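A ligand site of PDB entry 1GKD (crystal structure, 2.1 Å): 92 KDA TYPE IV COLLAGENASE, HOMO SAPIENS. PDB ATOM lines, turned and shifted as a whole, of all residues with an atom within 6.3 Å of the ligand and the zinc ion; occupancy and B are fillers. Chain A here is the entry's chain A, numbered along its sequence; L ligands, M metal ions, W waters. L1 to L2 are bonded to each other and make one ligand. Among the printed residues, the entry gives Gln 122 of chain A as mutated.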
ATOM      1  N   GLU A   6      -9.713 -20.218  -3.744  1.00  0.00           N
ATOM      2  CA  GLU A   6     -10.233 -19.588  -2.534  1.00  0.00           C
ATOM      3  C   GLU A   6     -11.615 -18.989  -2.820  1.00  0.00           C
ATOM      4  O   GLU A   6     -11.734 -17.786  -3.049  1.00  0.00           O
ATOM      5  CB  GLU A   6      -9.283 -18.491  -2.055  1.00  0.00           C
ATOM      6  CG  GLU A   6      -7.843 -18.949  -1.814  1.00  0.00           C
ATOM      7  CD  GLU A   6      -7.638 -19.597  -0.454  1.00  0.00           C
ATOM      8  OE1 GLU A   6      -7.521 -18.860   0.553  1.00  0.00           O
ATOM      9  OE2 GLU A   6      -7.602 -20.849  -0.389  1.00  0.00           O
ATOM     10  N   ASP A  80       8.833 -32.025  -4.232  1.00  0.00           N
ATOM     11  CA  ASP A  80       8.838 -30.813  -3.412  1.00  0.00           C
ATOM     12  C   ASP A  80       8.047 -29.681  -4.029  1.00  0.00           C
ATOM     13  O   ASP A  80       7.465 -29.827  -5.101  1.00  0.00           O
ATOM     14  CB  ASP A  80      10.261 -30.341  -3.122  1.00  0.00           C
ATOM     15  CG  ASP A  80      11.031 -31.312  -2.274  1.00  0.00           C
ATOM     16  OD1 ASP A  80      10.533 -31.675  -1.185  1.00  0.00           O
ATOM     17  OD2 ASP A  80      12.137 -31.723  -2.681  1.00  0.00           O
ATOM     18  N   GLY A  81       8.047 -28.539  -3.355  1.00  0.00           N
ATOM     19  CA  GLY A  81       7.299 -27.404  -3.851  1.00  0.00           C
ATOM     20  C   GLY A  81       5.840 -27.606  -3.487  1.00  0.00           C
ATOM     21  O   GLY A  81       5.539 -27.845  -2.322  1.00  0.00           O
ATOM     22  N   LEU A  82       4.948 -27.516  -4.474  1.00  0.00           N
ATOM     23  CA  LEU A  82       3.526 -27.692  -4.245  1.00  0.00           C
ATOM     24  C   LEU A  82       3.233 -29.138  -3.848  1.00  0.00           C
ATOM     25  O   LEU A  82       3.441 -30.039  -4.641  1.00  0.00           O
ATOM     26  CB  LEU A  82       2.754 -27.358  -5.513  1.00  0.00           C
ATOM     27  CG  LEU A  82       1.233 -27.395  -5.419  1.00  0.00           C
ATOM     28  CD1 LEU A  82       0.775 -26.348  -4.417  1.00  0.00           C
ATOM     29  CD2 LEU A  82       0.597 -27.141  -6.800  1.00  0.00           C
ATOM     30  N   LEU A  83       2.716 -29.361  -2.635  1.00  0.00           N
ATOM     31  CA  LEU A  83       2.417 -30.724  -2.205  1.00  0.00           C
ATOM     32  C   LEU A  83       1.079 -31.275  -2.685  1.00  0.00           C
ATOM     33  O   LEU A  83       0.969 -32.461  -3.023  1.00  0.00           O
ATOM     34  CB  LEU A  83       2.495 -30.816  -0.675  1.00  0.00           C
ATOM     35  CG  LEU A  83       3.841 -30.397  -0.062  1.00  0.00           C
ATOM     36  CD1 LEU A  83       3.783 -30.464   1.451  1.00  0.00           C
ATOM     37  CD2 LEU A  83       4.942 -31.310  -0.601  1.00  0.00           C
ATOM     38  N   ALA A  84       0.065 -30.415  -2.723  1.00  0.00           N
ATOM     39  CA  ALA A  84      -1.273 -30.817  -3.136  1.00  0.00           C
ATOM     40  C   ALA A  84      -2.178 -29.594  -3.176  1.00  0.00           C
ATOM     41  O   ALA A  84      -1.773 -28.506  -2.774  1.00  0.00           O
ATOM     42  CB  ALA A  84      -1.831 -31.842  -2.149  1.00  0.00           C
ATOM     43  N   HIS A  85      -3.400 -29.777  -3.675  1.00  0.00           N
ATOM     44  CA  HIS A  85      -4.346 -28.671  -3.734  1.00  0.00           C
ATOM     45  C   HIS A  85      -5.787 -29.162  -3.754  1.00  0.00           C
ATOM     46  O   HIS A  85      -6.047 -30.290  -4.117  1.00  0.00           O
ATOM     47  CB  HIS A  85      -4.059 -27.772  -4.942  1.00  0.00           C
ATOM     48  CG  HIS A  85      -4.172 -28.458  -6.271  1.00  0.00           C
ATOM     49  ND1 HIS A  85      -3.422 -28.075  -7.369  1.00  0.00           N
ATOM     50  CD2 HIS A  85      -4.999 -29.429  -6.705  1.00  0.00           C
ATOM     51  CE1 HIS A  85      -3.778 -28.789  -8.416  1.00  0.00           C
ATOM     52  NE2 HIS A  85      -4.735 -29.622  -8.039  1.00  0.00           N
ATOM     53  N   ALA A  86      -6.724 -28.319  -3.324  1.00  0.00           N
ATOM     54  CA  ALA A  86      -8.135 -28.701  -3.299  1.00  0.00           C
ATOM     55  C   ALA A  86      -8.994 -27.534  -3.754  1.00  0.00           C
ATOM     56  O   ALA A  86      -8.511 -26.401  -3.848  1.00  0.00           O
ATOM     57  CB  ALA A  86      -8.537 -29.149  -1.891  1.00  0.00           C
ATOM     58  N   TYR A 113       6.684 -36.645   3.374  1.00  0.00           N
ATOM     59  CA  TYR A 113       5.636 -35.825   3.953  1.00  0.00           C
ATOM     60  C   TYR A 113       4.474 -36.666   4.511  1.00  0.00           C
ATOM     61  O   TYR A 113       4.090 -37.673   3.928  1.00  0.00           O
ATOM     62  CB  TYR A 113       5.095 -34.872   2.903  1.00  0.00           C
ATOM     63  CG  TYR A 113       6.122 -33.914   2.357  1.00  0.00           C
ATOM     64  CD1 TYR A 113       6.416 -32.734   3.043  1.00  0.00           C
ATOM     65  CD2 TYR A 113       6.779 -34.167   1.162  1.00  0.00           C
ATOM     66  CE1 TYR A 113       7.347 -31.821   2.533  1.00  0.00           C
ATOM     67  CE2 TYR A 113       7.715 -33.273   0.636  1.00  0.00           C
ATOM     68  CZ  TYR A 113       7.993 -32.093   1.338  1.00  0.00           C
ATOM     69  OH  TYR A 113       8.908 -31.187   0.830  1.00  0.00           O
ATOM     70  N   LEU A 117      -1.406 -35.406   7.783  1.00  0.00           N
ATOM     71  CA  LEU A 117      -1.438 -33.975   8.033  1.00  0.00           C
ATOM     72  C   LEU A 117      -1.790 -33.141   6.802  1.00  0.00           C
ATOM     73  O   LEU A 117      -2.516 -32.158   6.902  1.00  0.00           O
ATOM     74  CB  LEU A 117      -0.094 -33.514   8.612  1.00  0.00           C
ATOM     75  CG  LEU A 117       0.246 -34.033  10.024  1.00  0.00           C
ATOM     76  CD1 LEU A 117       1.631 -33.543  10.460  1.00  0.00           C
ATOM     77  CD2 LEU A 117      -0.814 -33.523  11.012  1.00  0.00           C
ATOM     78  N   VAL A 118      -1.270 -33.530   5.643  1.00  0.00           N
ATOM     79  CA  VAL A 118      -1.553 -32.805   4.397  1.00  0.00           C
ATOM     80  C   VAL A 118      -3.027 -32.969   3.999  1.00  0.00           C
ATOM     81  O   VAL A 118      -3.657 -32.023   3.529  1.00  0.00           O
ATOM     82  CB  VAL A 118      -0.621 -33.280   3.241  1.00  0.00           C
ATOM     83  CG1 VAL A 118      -1.018 -32.614   1.929  1.00  0.00           C
ATOM     84  CG2 VAL A 118       0.836 -32.936   3.562  1.00  0.00           C
ATOM     85  N   ALA A 119      -3.566 -34.174   4.193  1.00  0.00           N
ATOM     86  CA  ALA A 119      -4.972 -34.454   3.868  1.00  0.00           C
ATOM     87  C   ALA A 119      -5.889 -33.590   4.742  1.00  0.00           C
ATOM     88  O   ALA A 119      -6.872 -33.022   4.267  1.00  0.00           O
ATOM     89  CB  ALA A 119      -5.280 -35.939   4.088  1.00  0.00           C
ATOM     90  N   HIS A 121      -5.339 -30.725   5.991  1.00  0.00           N
ATOM     91  CA  HIS A 121      -5.267 -29.369   5.450  1.00  0.00           C
ATOM     92  C   HIS A 121      -6.093 -29.233   4.167  1.00  0.00           C
ATOM     93  O   HIS A 121      -6.828 -28.257   4.001  1.00  0.00           O
ATOM     94  CB  HIS A 121      -3.812 -29.000   5.169  1.00  0.00           C
ATOM     95  CG  HIS A 121      -3.614 -27.615   4.623  1.00  0.00           C
ATOM     96  ND1 HIS A 121      -3.307 -26.530   5.410  1.00  0.00           N
ATOM     97  CD2 HIS A 121      -3.696 -27.143   3.353  1.00  0.00           C
ATOM     98  CE1 HIS A 121      -3.204 -25.454   4.651  1.00  0.00           C
ATOM     99  NE2 HIS A 121      -3.431 -25.798   3.399  1.00  0.00           N
ATOM    100  N   GLN A 122      -5.946 -30.188   3.251  1.00  0.00           N
ATOM    101  CA  GLN A 122      -6.707 -30.154   1.988  1.00  0.00           C
ATOM    102  C   GLN A 122      -8.214 -30.236   2.255  1.00  0.00           C
ATOM    103  O   GLN A 122      -9.006 -29.532   1.621  1.00  0.00           O
ATOM    104  CB  GLN A 122      -6.316 -31.319   1.068  1.00  0.00           C
ATOM    105  CG  GLN A 122      -4.841 -31.392   0.707  1.00  0.00           C
ATOM    106  CD  GLN A 122      -4.289 -30.074   0.202  1.00  0.00           C
ATOM    107  OE1 GLN A 122      -3.374 -29.500   0.813  1.00  0.00           O
ATOM    108  NE2 GLN A 122      -4.842 -29.579  -0.890  1.00  0.00           N
ATOM    109  N   HIS A 125      -9.857 -27.003   3.106  1.00  0.00           N
ATOM    110  CA  HIS A 125     -10.243 -26.198   1.942  1.00  0.00           C
ATOM    111  C   HIS A 125     -11.508 -26.735   1.294  1.00  0.00           C
ATOM    112  O   HIS A 125     -12.376 -25.969   0.872  1.00  0.00           O
ATOM    113  CB  HIS A 125      -9.135 -26.170   0.901  1.00  0.00           C
ATOM    114  CG  HIS A 125      -7.970 -25.315   1.274  1.00  0.00           C
ATOM    115  ND1 HIS A 125      -8.110 -23.993   1.649  1.00  0.00           N
ATOM    116  CD2 HIS A 125      -6.649 -25.567   1.290  1.00  0.00           C
ATOM    117  CE1 HIS A 125      -6.918 -23.476   1.875  1.00  0.00           C
ATOM    118  NE2 HIS A 125      -6.018 -24.411   1.661  1.00  0.00           N
ATOM    119  N   HIS A 131      -6.890 -19.889   4.080  1.00  0.00           N
ATOM    120  CA  HIS A 131      -5.613 -19.974   4.770  1.00  0.00           C
ATOM    121  C   HIS A 131      -5.601 -19.120   6.050  1.00  0.00           C
ATOM    122  O   HIS A 131      -6.188 -18.050   6.089  1.00  0.00           O
ATOM    123  CB  HIS A 131      -4.490 -19.513   3.844  1.00  0.00           C
ATOM    124  CG  HIS A 131      -4.035 -20.551   2.877  1.00  0.00           C
ATOM    125  ND1 HIS A 131      -3.428 -20.231   1.676  1.00  0.00           N
ATOM    126  CD2 HIS A 131      -4.024 -21.903   2.947  1.00  0.00           C
ATOM    127  CE1 HIS A 131      -3.065 -21.340   1.055  1.00  0.00           C
ATOM    128  NE2 HIS A 131      -3.423 -22.372   1.798  1.00  0.00           N
ATOM    129  N   LEU A 138      -3.291 -25.327  11.540  1.00  0.00           N
ATOM    130  CA  LEU A 138      -3.211 -26.330  10.491  1.00  0.00           C
ATOM    131  C   LEU A 138      -3.432 -25.715   9.115  1.00  0.00           C
ATOM    132  O   LEU A 138      -2.893 -26.183   8.120  1.00  0.00           O
ATOM    133  CB  LEU A 138      -4.239 -27.443  10.719  1.00  0.00           C
ATOM    134  CG  LEU A 138      -4.287 -28.531   9.646  1.00  0.00           C
ATOM    135  CD1 LEU A 138      -3.021 -29.355   9.714  1.00  0.00           C
ATOM    136  CD2 LEU A 138      -5.491 -29.446   9.859  1.00  0.00           C
ATOM    137  N   MET A 139      -4.245 -24.669   9.050  1.00  0.00           N
ATOM    138  CA  MET A 139      -4.534 -24.025   7.777  1.00  0.00           C
ATOM    139  C   MET A 139      -3.461 -23.023   7.343  1.00  0.00           C
ATOM    140  O   MET A 139      -3.645 -22.266   6.398  1.00  0.00           O
ATOM    141  CB  MET A 139      -5.915 -23.355   7.807  1.00  0.00           C
ATOM    142  CG  MET A 139      -7.085 -24.333   7.924  1.00  0.00           C
ATOM    143  SD  MET A 139      -6.936 -25.797   6.833  1.00  0.00           S
ATOM    144  CE  MET A 139      -7.016 -25.028   5.214  1.00  0.00           C
ATOM    145  N   TYR A 140      -2.334 -23.028   8.061  1.00  0.00           N
ATOM    146  CA  TYR A 140      -1.214 -22.151   7.711  1.00  0.00           C
ATOM    147  C   TYR A 140      -0.711 -22.707   6.369  1.00  0.00           C
ATOM    148  O   TYR A 140      -0.555 -23.913   6.207  1.00  0.00           O
ATOM    149  CB  TYR A 140      -0.149 -22.223   8.812  1.00  0.00           C
ATOM    150  CG  TYR A 140       0.996 -21.251   8.636  1.00  0.00           C
ATOM    151  CD1 TYR A 140       0.754 -19.876   8.543  1.00  0.00           C
ATOM    152  CD2 TYR A 140       2.306 -21.703   8.552  1.00  0.00           C
ATOM    153  CE1 TYR A 140       1.799 -18.981   8.347  1.00  0.00           C
ATOM    154  CE2 TYR A 140       3.356 -20.821   8.354  1.00  0.00           C
ATOM    155  CZ  TYR A 140       3.107 -19.463   8.252  1.00  0.00           C
ATOM    156  OH  TYR A 140       4.152 -18.595   8.037  1.00  0.00           O
ATOM    157  N   PRO A 141      -0.455 -21.824   5.391  1.00  0.00           N
ATOM    158  CA  PRO A 141       0.019 -22.191   4.038  1.00  0.00           C
ATOM    159  C   PRO A 141       1.359 -22.929   3.869  1.00  0.00           C
ATOM    160  O   PRO A 141       1.709 -23.324   2.759  1.00  0.00           O
ATOM    161  CB  PRO A 141      -0.014 -20.856   3.299  1.00  0.00           C
ATOM    162  CG  PRO A 141       0.287 -19.878   4.379  1.00  0.00           C
ATOM    163  CD  PRO A 141      -0.568 -20.364   5.514  1.00  0.00           C
ATOM    164  N   MET A 142       2.093 -23.120   4.961  1.00  0.00           N
ATOM    165  CA  MET A 142       3.388 -23.808   4.901  1.00  0.00           C
ATOM    166  C   MET A 142       3.324 -25.152   5.629  1.00  0.00           C
ATOM    167  O   MET A 142       2.747 -25.270   6.713  1.00  0.00           O
ATOM    168  CB  MET A 142       4.460 -22.920   5.538  1.00  0.00           C
ATOM    169  CG  MET A 142       5.836 -23.572   5.670  1.00  0.00           C
ATOM    170  SD  MET A 142       7.015 -22.608   6.681  1.00  0.00           S
ATOM    171  CE  MET A 142       6.881 -23.436   8.304  1.00  0.00           C
ATOM    172  N   TYR A 143       3.917 -26.185   5.029  1.00  0.00           N
ATOM    173  CA  TYR A 143       3.931 -27.496   5.665  1.00  0.00           C
ATOM    174  C   TYR A 143       4.870 -27.536   6.868  1.00  0.00           C
ATOM    175  O   TYR A 143       5.999 -27.047   6.799  1.00  0.00           O
ATOM    176  CB  TYR A 143       4.387 -28.583   4.673  1.00  0.00           C
ATOM    177  CG  TYR A 143       4.543 -29.947   5.332  1.00  0.00           C
ATOM    178  CD1 TYR A 143       3.434 -30.734   5.613  1.00  0.00           C
ATOM    179  CD2 TYR A 143       5.791 -30.421   5.734  1.00  0.00           C
ATOM    180  CE1 TYR A 143       3.547 -31.952   6.263  1.00  0.00           C
ATOM    181  CE2 TYR A 143       5.925 -31.641   6.393  1.00  0.00           C
ATOM    182  CZ  TYR A 143       4.795 -32.410   6.659  1.00  0.00           C
ATOM    183  OH  TYR A 143       4.887 -33.627   7.301  1.00  0.00           O
ATOM    184  N   ARG A 144       4.405 -28.122   7.960  1.00  0.00           N
ATOM    185  CA  ARG A 144       5.230 -28.276   9.158  1.00  0.00           C
ATOM    186  C   ARG A 144       4.758 -29.509   9.926  1.00  0.00           C
ATOM    187  O   ARG A 144       3.589 -29.631  10.270  1.00  0.00           O
ATOM    188  CB  ARG A 144       5.162 -27.034  10.059  1.00  0.00           C
ATOM    189  CG  ARG A 144       3.778 -26.606  10.476  1.00  0.00           C
ATOM    190  CD  ARG A 144       3.853 -25.488  11.513  1.00  0.00           C
ATOM    191  NE  ARG A 144       3.751 -25.987  12.888  1.00  0.00           N
ATOM    192  CZ  ARG A 144       3.947 -25.243  13.976  1.00  0.00           C
ATOM    193  NH1 ARG A 144       4.285 -23.962  13.865  1.00  0.00           N
ATOM    194  NH2 ARG A 144       3.810 -25.789  15.186  1.00  0.00           N
HETATM  195  C1  LIG L   1       0.603 -26.998   3.826  1.00  0.00           C
HETATM  196  C2  LIG L   1       0.776 -28.023   2.687  1.00  0.00           C
HETATM  197  C3  LIG L   1      -0.275 -25.877  -0.591  1.00  0.00           C
HETATM  198  C4  LIG L   1       0.599 -26.226   0.660  1.00  0.00           C
HETATM  199  C5  LIG L   1       0.059 -27.524   1.402  1.00  0.00           C
HETATM  200  C6  LIG L   1       0.103 -29.284   3.191  1.00  0.00           C
HETATM  201  C7  LIG L   1       2.004 -26.436   0.057  1.00  0.00           C
HETATM  202  C8  LIG L   1      -2.704 -26.323  -0.694  1.00  0.00           C
HETATM  203  O1  LIG L   1      -1.874 -24.509   0.403  1.00  0.00           O
HETATM  204  N1  LIG L   1      -1.665 -25.569  -0.292  1.00  0.00           N
HETATM  205  O2  LIG L   1      -3.832 -26.081  -0.460  1.00  0.00           O
HETATM  206  O3  LIG L   1       2.163 -27.289  -0.856  1.00  0.00           O
HETATM  207  C1  LG2 L   2       4.100 -23.562  -1.359  1.00  0.00           C
HETATM  208  C2  LG2 L   2       4.912 -23.252   0.956  1.00  0.00           C
HETATM  209  C3  LG2 L   2       4.963 -24.238  -0.269  1.00  0.00           C
HETATM  210  C4  LG2 L   2       4.429 -25.718   0.059  1.00  0.00           C
HETATM  211  C5  LG2 L   2       6.465 -24.252  -0.748  1.00  0.00           C
HETATM  212  C6  LG2 L   2       5.286 -26.468   1.182  1.00  0.00           C
HETATM  213  O1  LG2 L   2       5.159 -26.174   2.402  1.00  0.00           O
HETATM  214  N1  LG2 L   2       2.991 -25.680   0.528  1.00  0.00           N
HETATM  215  N2  LG2 L   2       6.137 -27.417   0.705  1.00  0.00           N
HETATM  216  C7  LG2 L   2       7.040 -28.250   1.540  1.00  0.00           C
HETATM  217 ZN    ZN M   1      -3.685 -24.681   1.540  1.00  0.00          ZN
HETATM  218  O   HOH W   1       0.284 -22.644   0.209  1.00  0.00           O
HETATM  219  O   HOH W   2      -5.751 -25.943  -2.415  1.00  0.00           O
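OH of Tyr 113 is in hydrogen-bond range of OD1 of Asp 80 (2.6 Å).
The side-chain amide nitrogen of Gln 122 sits close to the backbone NH of His 85, at 3.1 Å.
N of Ala 86 sits close to NE2 of Gln 122 (3.3 Å).
ND1 of His 121 sits at hydrogen-bond distance from O of Leu 138 (2.8 Å).
Within 4 Å of the zinc ion: His 121, His 125 and His 131.
The zinc ion is bound by O1 of LIG L1, NE2 of His 121, NE2 of His 131, NE2 of His 125 and O2 of LIG L1.
The zinc ion has five donor atoms within binding distance.
N of Tyr 143 lies within hydrogen-bond range of O1 of LG2 L2, 2.9 Å away.
O of Gly 81 sits at hydrogen-bond distance from N2 of LG2 L2.
The backbone NH (N) of Leu 83 sits at hydrogen-bond distance from an oxygen (O3) of LIG L1 (2.8 Å).
The backbone carbonyl oxygen (O) of Pro 141 sits at hydrogen-bond distance from a nitrogen (N1) of LG2 L2, at 3.5 Å.
Merely in contact with the ligand: Leu 82, Ala 84, Tyr 113, Val 118, Gln 122 and Met 142.
13 residues have an atom within 4 Å of the ligand: Gly 81, Leu 82, Leu 83, Ala 84, Tyr 113, Val 118, His 121, Gln 122, His 125, His 131, Pro 141, Met 142 and Tyr 143.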
